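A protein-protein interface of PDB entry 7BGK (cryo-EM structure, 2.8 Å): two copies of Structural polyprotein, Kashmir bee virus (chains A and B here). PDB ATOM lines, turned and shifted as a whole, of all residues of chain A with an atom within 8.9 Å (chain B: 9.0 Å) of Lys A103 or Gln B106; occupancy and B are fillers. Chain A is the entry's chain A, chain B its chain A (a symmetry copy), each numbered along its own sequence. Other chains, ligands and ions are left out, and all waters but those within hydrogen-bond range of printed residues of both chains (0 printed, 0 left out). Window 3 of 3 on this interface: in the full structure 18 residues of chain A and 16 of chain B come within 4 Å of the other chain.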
ATOM      1  N   ASN A  98       2.514  -8.881   2.280  1.00  0.00           N
ATOM      2  CA  ASN A  98       3.436  -8.035   1.539  1.00  0.00           C
ATOM      3  C   ASN A  98       2.690  -6.961   0.763  1.00  0.00           C
ATOM      4  O   ASN A  98       1.698  -7.241   0.084  1.00  0.00           O
ATOM      5  CB  ASN A  98       4.268  -8.883   0.584  1.00  0.00           C
ATOM      6  CG  ASN A  98       5.488  -8.163   0.079  1.00  0.00           C
ATOM      7  OD1 ASN A  98       6.183  -7.484   0.833  1.00  0.00           O
ATOM      8  ND2 ASN A  98       5.763  -8.311  -1.206  1.00  0.00           N
ATOM      9  N   THR A  99       3.176  -5.724   0.868  1.00  0.00           N
ATOM     10  CA  THR A  99       2.662  -4.595   0.105  1.00  0.00           C
ATOM     11  C   THR A  99       3.806  -3.781  -0.480  1.00  0.00           C
ATOM     12  O   THR A  99       3.711  -2.557  -0.596  1.00  0.00           O
ATOM     13  CB  THR A  99       1.764  -3.711   0.966  1.00  0.00           C
ATOM     14  OG1 THR A  99       2.544  -3.019   1.945  1.00  0.00           O
ATOM     15  CG2 THR A  99       0.719  -4.534   1.667  1.00  0.00           C
ATOM     16  N   THR A 100       4.886  -4.447  -0.854  1.00  0.00           N
ATOM     17  CA  THR A 100       6.069  -3.766  -1.358  1.00  0.00           C
ATOM     18  C   THR A 100       5.831  -3.263  -2.777  1.00  0.00           C
ATOM     19  O   THR A 100       5.580  -4.073  -3.678  1.00  0.00           O
ATOM     20  CB  THR A 100       7.258  -4.712  -1.318  1.00  0.00           C
ATOM     21  OG1 THR A 100       7.346  -5.307  -0.022  1.00  0.00           O
ATOM     22  CG2 THR A 100       8.536  -3.974  -1.604  1.00  0.00           C
ATOM     23  N   PRO A 101       5.893  -1.951  -3.020  1.00  0.00           N
ATOM     24  CA  PRO A 101       5.536  -1.425  -4.345  1.00  0.00           C
ATOM     25  C   PRO A 101       6.653  -1.477  -5.373  1.00  0.00           C
ATOM     26  O   PRO A 101       6.363  -1.390  -6.572  1.00  0.00           O
ATOM     27  CB  PRO A 101       5.139   0.022  -4.045  1.00  0.00           C
ATOM     28  CG  PRO A 101       5.934   0.380  -2.855  1.00  0.00           C
ATOM     29  CD  PRO A 101       6.151  -0.867  -2.058  1.00  0.00           C
ATOM     30  N   LEU A 102       7.906  -1.601  -4.949  1.00  0.00           N
ATOM     31  CA  LEU A 102       9.059  -1.552  -5.833  1.00  0.00           C
ATOM     32  C   LEU A 102       9.805  -2.880  -5.816  1.00  0.00           C
ATOM     33  O   LEU A 102       9.740  -3.639  -4.846  1.00  0.00           O
ATOM     34  CB  LEU A 102       9.996  -0.426  -5.387  1.00  0.00           C
ATOM     35  CG  LEU A 102       9.444   0.993  -5.525  1.00  0.00           C
ATOM     36  CD1 LEU A 102      10.384   1.975  -4.886  1.00  0.00           C
ATOM     37  CD2 LEU A 102       9.288   1.350  -6.989  1.00  0.00           C
ATOM     38  N   LYS A 103      10.519  -3.151  -6.908  1.00  0.00           N
ATOM     39  CA  LYS A 103      11.327  -4.356  -7.048  1.00  0.00           C
ATOM     40  C   LYS A 103      12.783  -4.004  -6.776  1.00  0.00           C
ATOM     41  O   LYS A 103      13.360  -3.160  -7.468  1.00  0.00           O
ATOM     42  CB  LYS A 103      11.183  -4.950  -8.448  1.00  0.00           C
ATOM     43  CG  LYS A 103      11.683  -6.384  -8.569  1.00  0.00           C
ATOM     44  CD  LYS A 103      13.003  -6.493  -9.317  1.00  0.00           C
ATOM     45  CE  LYS A 103      13.212  -7.903  -9.837  1.00  0.00           C
ATOM     46  NZ  LYS A 103      14.525  -8.062 -10.521  1.00  0.00           N
ATOM     47  N   GLN A 104      13.375  -4.650  -5.774  1.00  0.00           N
ATOM     48  CA  GLN A 104      14.765  -4.409  -5.408  1.00  0.00           C
ATOM     49  C   GLN A 104      15.692  -5.498  -5.921  1.00  0.00           C
ATOM     50  O   GLN A 104      16.727  -5.205  -6.525  1.00  0.00           O
ATOM     51  CB  GLN A 104      14.898  -4.303  -3.888  1.00  0.00           C
ATOM     52  CG  GLN A 104      14.078  -3.192  -3.277  1.00  0.00           C
ATOM     53  CD  GLN A 104      12.635  -3.590  -3.065  1.00  0.00           C
ATOM     54  OE1 GLN A 104      12.183  -4.623  -3.557  1.00  0.00           O
ATOM     55  NE2 GLN A 104      11.899  -2.766  -2.335  1.00  0.00           N
ATOM     56  N   SER A 105      15.335  -6.758  -5.689  1.00  0.00           N
ATOM     57  CA  SER A 105      16.141  -7.890  -6.111  1.00  0.00           C
ATOM     58  C   SER A 105      15.265  -8.923  -6.804  1.00  0.00           C
ATOM     59  O   SER A 105      14.061  -9.024  -6.560  1.00  0.00           O
ATOM     60  CB  SER A 105      16.886  -8.553  -4.945  1.00  0.00           C
ATOM     61  OG  SER A 105      17.851  -7.680  -4.387  1.00  0.00           O
ATOM     62  N   GLN A 106      15.912  -9.682  -7.682  1.00  0.00           N
ATOM     63  CA  GLN A 106      15.270 -10.769  -8.412  1.00  0.00           C
ATOM     64  C   GLN A 106      14.554 -11.728  -7.474  1.00  0.00           C
ATOM     65  O   GLN A 106      13.463 -12.224  -7.780  1.00  0.00           O
ATOM     66  CB  GLN A 106      16.362 -11.529  -9.160  1.00  0.00           C
ATOM     67  CG  GLN A 106      17.147 -10.854 -10.299  1.00  0.00           C
ATOM     68  CD  GLN A 106      16.454 -10.335 -11.525  1.00  0.00           C
ATOM     69  OE1 GLN A 106      15.542 -10.939 -12.055  1.00  0.00           O
ATOM     70  NE2 GLN A 106      16.924  -9.174 -12.025  1.00  0.00           N
ATOM     71  N   THR A 107      15.135 -11.967  -6.307  1.00  0.00           N
ATOM     72  CA  THR A 107      14.618 -12.936  -5.353  1.00  0.00           C
ATOM     73  C   THR A 107      14.447 -12.239  -4.018  1.00  0.00           C
ATOM     74  O   THR A 107      15.431 -11.957  -3.329  1.00  0.00           O
ATOM     75  CB  THR A 107      15.556 -14.133  -5.241  1.00  0.00           C
ATOM     76  OG1 THR A 107      15.691 -14.755  -6.524  1.00  0.00           O
ATOM     77  CG2 THR A 107      15.020 -15.146  -4.268  1.00  0.00           C
ATOM     78  N   CYS A 108      13.200 -11.968  -3.653  1.00  0.00           N
ATOM     79  CA  CYS A 108      12.881 -11.384  -2.365  1.00  0.00           C
ATOM     80  C   CYS A 108      12.386 -12.479  -1.443  1.00  0.00           C
ATOM     81  O   CYS A 108      11.565 -13.309  -1.843  1.00  0.00           O
ATOM     82  CB  CYS A 108      11.800 -10.312  -2.484  1.00  0.00           C
ATOM     83  SG  CYS A 108      11.840  -9.231  -3.893  1.00  0.00           S
ATOM     84  N   PRO A 135       7.731 -13.631  -0.888  1.00  0.00           N
ATOM     85  CA  PRO A 135       6.499 -12.861  -1.103  1.00  0.00           C
ATOM     86  C   PRO A 135       5.933 -12.945  -2.505  1.00  0.00           C
ATOM     87  O   PRO A 135       4.778 -12.555  -2.704  1.00  0.00           O
ATOM     88  CB  PRO A 135       6.928 -11.432  -0.772  1.00  0.00           C
ATOM     89  CG  PRO A 135       8.036 -11.592   0.166  1.00  0.00           C
ATOM     90  CD  PRO A 135       8.771 -12.806  -0.256  1.00  0.00           C
ATOM     91  N   VAL A 136       6.698 -13.421  -3.479  1.00  0.00           N
ATOM     92  CA  VAL A 136       6.193 -13.474  -4.843  1.00  0.00           C
ATOM     93  C   VAL A 136       5.328 -14.709  -5.053  1.00  0.00           C
ATOM     94  O   VAL A 136       4.340 -14.666  -5.795  1.00  0.00           O
ATOM     95  CB  VAL A 136       7.369 -13.411  -5.830  1.00  0.00           C
ATOM     96  CG1 VAL A 136       6.902 -13.599  -7.249  1.00  0.00           C
ATOM     97  CG2 VAL A 136       8.067 -12.081  -5.696  1.00  0.00           C
ATOM     98  N   VAL A 174      15.322  -7.118   1.363  1.00  0.00           N
ATOM     99  CA  VAL A 174      14.980  -5.932   0.594  1.00  0.00           C
ATOM    100  C   VAL A 174      14.012  -5.100   1.419  1.00  0.00           C
ATOM    101  O   VAL A 174      13.410  -5.577   2.381  1.00  0.00           O
ATOM    102  CB  VAL A 174      14.373  -6.276  -0.785  1.00  0.00           C
ATOM    103  CG1 VAL A 174      15.341  -7.095  -1.596  1.00  0.00           C
ATOM    104  CG2 VAL A 174      13.073  -7.014  -0.634  1.00  0.00           C
ATOM    105  N   GLY A 175      13.869  -3.839   1.033  1.00  0.00           N
ATOM    106  CA  GLY A 175      12.926  -2.968   1.700  1.00  0.00           C
ATOM    107  C   GLY A 175      11.505  -3.328   1.339  1.00  0.00           C
ATOM    108  O   GLY A 175      11.053  -3.073   0.219  1.00  0.00           O
ATOM    109  N   LYS B 103       0.090  -2.061 -15.301  1.00  0.00           N
ATOM    110  CA  LYS B 103       0.832  -2.375 -14.087  1.00  0.00           C
ATOM    111  C   LYS B 103       1.184  -1.075 -13.379  1.00  0.00           C
ATOM    112  O   LYS B 103       1.868  -0.219 -13.950  1.00  0.00           O
ATOM    113  CB  LYS B 103       2.104  -3.157 -14.413  1.00  0.00           C
ATOM    114  CG  LYS B 103       2.739  -3.840 -13.207  1.00  0.00           C
ATOM    115  CD  LYS B 103       4.009  -3.150 -12.734  1.00  0.00           C
ATOM    116  CE  LYS B 103       4.852  -4.092 -11.895  1.00  0.00           C
ATOM    117  NZ  LYS B 103       6.075  -3.430 -11.361  1.00  0.00           N
ATOM    118  N   GLN B 104       0.723  -0.928 -12.139  1.00  0.00           N
ATOM    119  CA  GLN B 104       0.988   0.268 -11.348  1.00  0.00           C
ATOM    120  C   GLN B 104       2.083   0.046 -10.319  1.00  0.00           C
ATOM    121  O   GLN B 104       3.014   0.848 -10.214  1.00  0.00           O
ATOM    122  CB  GLN B 104      -0.289   0.724 -10.641  1.00  0.00           C
ATOM    123  CG  GLN B 104      -1.425   1.054 -11.579  1.00  0.00           C
ATOM    124  CD  GLN B 104      -2.182  -0.177 -12.025  1.00  0.00           C
ATOM    125  OE1 GLN B 104      -1.743  -1.305 -11.803  1.00  0.00           O
ATOM    126  NE2 GLN B 104      -3.321   0.032 -12.665  1.00  0.00           N
ATOM    127  N   SER B 105       1.986  -1.037  -9.553  1.00  0.00           N
ATOM    128  CA  SER B 105       2.958  -1.355  -8.521  1.00  0.00           C
ATOM    129  C   SER B 105       3.377  -2.813  -8.632  1.00  0.00           C
ATOM    130  O   SER B 105       2.639  -3.666  -9.131  1.00  0.00           O
ATOM    131  CB  SER B 105       2.427  -1.083  -7.107  1.00  0.00           C
ATOM    132  OG  SER B 105       2.199   0.299  -6.898  1.00  0.00           O
ATOM    133  N   GLN B 106       4.591  -3.067  -8.155  1.00  0.00           N
ATOM    134  CA  GLN B 106       5.160  -4.409  -8.115  1.00  0.00           C
ATOM    135  C   GLN B 106       4.226  -5.393  -7.431  1.00  0.00           C
ATOM    136  O   GLN B 106       4.099  -6.550  -7.850  1.00  0.00           O
ATOM    137  CB  GLN B 106       6.464  -4.332  -7.326  1.00  0.00           C
ATOM    138  CG  GLN B 106       7.664  -3.537  -7.871  1.00  0.00           C
ATOM    139  CD  GLN B 106       8.300  -3.884  -9.185  1.00  0.00           C
ATOM    140  OE1 GLN B 106       8.471  -5.036  -9.533  1.00  0.00           O
ATOM    141  NE2 GLN B 106       8.701  -2.844  -9.944  1.00  0.00           N
ATOM    142  N   THR B 107       3.530  -4.938  -6.398  1.00  0.00           N
ATOM    143  CA  THR B 107       2.675  -5.790  -5.587  1.00  0.00           C
ATOM    144  C   THR B 107       1.294  -5.165  -5.539  1.00  0.00           C
ATOM    145  O   THR B 107       1.085  -4.158  -4.857  1.00  0.00           O
ATOM    146  CB  THR B 107       3.257  -5.959  -4.188  1.00  0.00           C
ATOM    147  OG1 THR B 107       4.560  -6.547  -4.281  1.00  0.00           O
ATOM    148  CG2 THR B 107       2.385  -6.852  -3.348  1.00  0.00           C
ATOM    149  N   CYS B 108       0.355  -5.764  -6.260  1.00  0.00           N
ATOM    150  CA  CYS B 108      -1.028  -5.329  -6.242  1.00  0.00           C
ATOM    151  C   CYS B 108      -1.820  -6.259  -5.347  1.00  0.00           C
ATOM    152  O   CYS B 108      -1.672  -7.482  -5.429  1.00  0.00           O
ATOM    153  CB  CYS B 108      -1.644  -5.345  -7.639  1.00  0.00           C
ATOM    154  SG  CYS B 108      -0.635  -4.830  -9.008  1.00  0.00           S
ATOM    155  N   TYR B 109      -2.650  -5.678  -4.489  1.00  0.00           N
ATOM    156  CA  TYR B 109      -3.451  -6.453  -3.564  1.00  0.00           C
ATOM    157  C   TYR B 109      -4.828  -5.827  -3.453  1.00  0.00           C
ATOM    158  O   TYR B 109      -4.993  -4.611  -3.562  1.00  0.00           O
ATOM    159  CB  TYR B 109      -2.795  -6.564  -2.180  1.00  0.00           C
ATOM    160  CG  TYR B 109      -2.629  -5.274  -1.413  1.00  0.00           C
ATOM    161  CD1 TYR B 109      -1.432  -4.581  -1.435  1.00  0.00           C
ATOM    162  CD2 TYR B 109      -3.656  -4.773  -0.633  1.00  0.00           C
ATOM    163  CE1 TYR B 109      -1.275  -3.419  -0.727  1.00  0.00           C
ATOM    164  CE2 TYR B 109      -3.506  -3.614   0.077  1.00  0.00           C
ATOM    165  CZ  TYR B 109      -2.313  -2.940   0.030  1.00  0.00           C
ATOM    166  OH  TYR B 109      -2.158  -1.776   0.741  1.00  0.00           O
ATOM    167  N   TYR B 134      -4.366 -11.286  -3.804  1.00  0.00           N
ATOM    168  CA  TYR B 134      -3.344 -10.747  -4.693  1.00  0.00           C
ATOM    169  C   TYR B 134      -3.689 -11.111  -6.127  1.00  0.00           C
ATOM    170  O   TYR B 134      -3.519 -12.279  -6.526  1.00  0.00           O
ATOM    171  CB  TYR B 134      -1.968 -11.277  -4.305  1.00  0.00           C
ATOM    172  CG  TYR B 134      -1.436 -10.628  -3.056  1.00  0.00           C
ATOM    173  CD1 TYR B 134      -0.530  -9.586  -3.128  1.00  0.00           C
ATOM    174  CD2 TYR B 134      -1.861 -11.035  -1.806  1.00  0.00           C
ATOM    175  CE1 TYR B 134      -0.053  -8.985  -1.992  1.00  0.00           C
ATOM    176  CE2 TYR B 134      -1.390 -10.439  -0.669  1.00  0.00           C
ATOM    177  CZ  TYR B 134      -0.490  -9.416  -0.766  1.00  0.00           C
ATOM    178  OH  TYR B 134      -0.030  -8.829   0.377  1.00  0.00           O
ATOM    179  N   PRO B 135      -4.173 -10.164  -6.934  1.00  0.00           N
ATOM    180  CA  PRO B 135      -4.711 -10.515  -8.256  1.00  0.00           C
ATOM    181  C   PRO B 135      -3.737 -11.231  -9.167  1.00  0.00           C
ATOM    182  O   PRO B 135      -4.172 -11.792 -10.180  1.00  0.00           O
ATOM    183  CB  PRO B 135      -5.103  -9.155  -8.835  1.00  0.00           C
ATOM    184  CG  PRO B 135      -5.378  -8.327  -7.665  1.00  0.00           C
ATOM    185  CD  PRO B 135      -4.423  -8.750  -6.617  1.00  0.00           C
ATOM    186  N   VAL B 136      -2.446 -11.224  -8.862  1.00  0.00           N
ATOM    187  CA  VAL B 136      -1.485 -11.868  -9.744  1.00  0.00           C
ATOM    188  C   VAL B 136      -1.435 -13.369  -9.488  1.00  0.00           C
ATOM    189  O   VAL B 136      -1.252 -14.160 -10.419  1.00  0.00           O
ATOM    190  CB  VAL B 136      -0.108 -11.203  -9.580  1.00  0.00           C
ATOM    191  CG1 VAL B 136       0.947 -11.928 -10.374  1.00  0.00           C
ATOM    192  CG2 VAL B 136      -0.188  -9.766 -10.031  1.00  0.00           C
ATOM    193  N   ASN B 173      -4.915  -0.910  -3.650  1.00  0.00           N
ATOM    194  CA  ASN B 173      -3.774  -0.008  -3.613  1.00  0.00           C
ATOM    195  C   ASN B 173      -3.425   0.555  -4.980  1.00  0.00           C
ATOM    196  O   ASN B 173      -2.585   1.455  -5.065  1.00  0.00           O
ATOM    197  CB  ASN B 173      -2.569  -0.733  -3.030  1.00  0.00           C
ATOM    198  CG  ASN B 173      -2.240  -1.998  -3.772  1.00  0.00           C
ATOM    199  OD1 ASN B 173      -3.128  -2.704  -4.238  1.00  0.00           O
ATOM    200  ND2 ASN B 173      -0.960  -2.296  -3.887  1.00  0.00           N
ATOM    201  N   VAL B 174      -4.046   0.048  -6.046  1.00  0.00           N
ATOM    202  CA  VAL B 174      -3.786   0.497  -7.405  1.00  0.00           C
ATOM    203  C   VAL B 174      -5.116   0.570  -8.138  1.00  0.00           C
ATOM    204  O   VAL B 174      -6.121   0.006  -7.706  1.00  0.00           O
ATOM    205  CB  VAL B 174      -2.797  -0.426  -8.152  1.00  0.00           C
ATOM    206  CG1 VAL B 174      -1.481  -0.487  -7.423  1.00  0.00           C
ATOM    207  CG2 VAL B 174      -3.362  -1.808  -8.313  1.00  0.00           C
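N of Asn A98 lies within hydrogen-bond range of OH of Tyr B134, 3.2 Å away.
The backbone carbonyl oxygen of Thr A100 is in hydrogen-bond range of the side-chain hydroxyl of Thr B107.
The backbone carbonyl oxygen (O) of Pro A101 lies close to the backbone NH (N) of Gln B106, at 2.9 Å.
Of the printed residues of chain B, Asn A98 touches Thr B107 (3.5 Å) and Tyr B134 (2.4 Å).
Of the printed residues of chain B, Thr A100 touches Gln B106 and Thr B107.
Of the printed residues of chain B, Leu A102 touches Gln B106.
Of chain B, only Gln B106 comes within 4 Å of Lys A103.
No residue of chain B comes within 4 Å of Gln A104.
Cys A108 touches none of the printed residues of chain B.
Val A174 touches none of the printed residues of chain B.
Of chain A, only Thr A100, Pro A101, Leu A102 and Lys A103 come within 4 Å of Gln B106.
Thr B107 touches just these residues of chain A: Asn A98 (3.5 Å) and Thr A100 (2.7 Å).
Printed residues of chain A within 4 Å of Tyr B109: Thr A99 (3.3 Å).
Printed residues of chain A within 4 Å of Tyr B134: Asn A98.
Lys A103 touches Gln B106, but with the chains exchanged Gln A106 does not touch Lys B103 (12.0 Å).
Of the 9 pairs that touch across the chains among the printed residues, none has its exchanged pair printed and touching as well.
Of the 15 printed residues of chain A, 6 touch a printed residue of chain B.
Among the printed residues, no Asp or Glu carboxylate lies within 4 Å of a Lys or Arg side-chain nitrogen of the other chain.
O of Asn A98 touches CG2 of Thr B107, 3.5 Å away.
Tyr B109 touches Thr A99 (CE1 to CG2, 3.3 Å).
O of Thr A100 touches CB of Gln B106, 3.8 Å away.
Pro A101 touches Ser B105.
Gln B106 touches Leu A102 (CG to C, 3.0 Å).
Lys A103 touches Gln B106.
The side-chain amide oxygen (OE1) of Gln A104 lies close to the backbone carbonyl oxygen (O) of Leu A102, 2.9 Å away.
The side-chain amide nitrogen (NE2) of Gln A106 lies close to the side-chain amino group (NZ) of Lys A103 (3.0 Å).
The side-chain amide nitrogen (NE2) of Gln B106 sits close to the side-chain amino group (NZ) of Lys B103 (3.0 Å).
The backbone carbonyl oxygen of Ser B105 lies within hydrogen-bond range of the side-chain sulfur of Cys B108, 3.5 Å away.
ND2 of Asn B173 is in hydrogen-bond range of O of Thr B107 (2.9 Å).
O of Tyr B109 sits close to OD1 of Asn B173 (2.8 Å).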
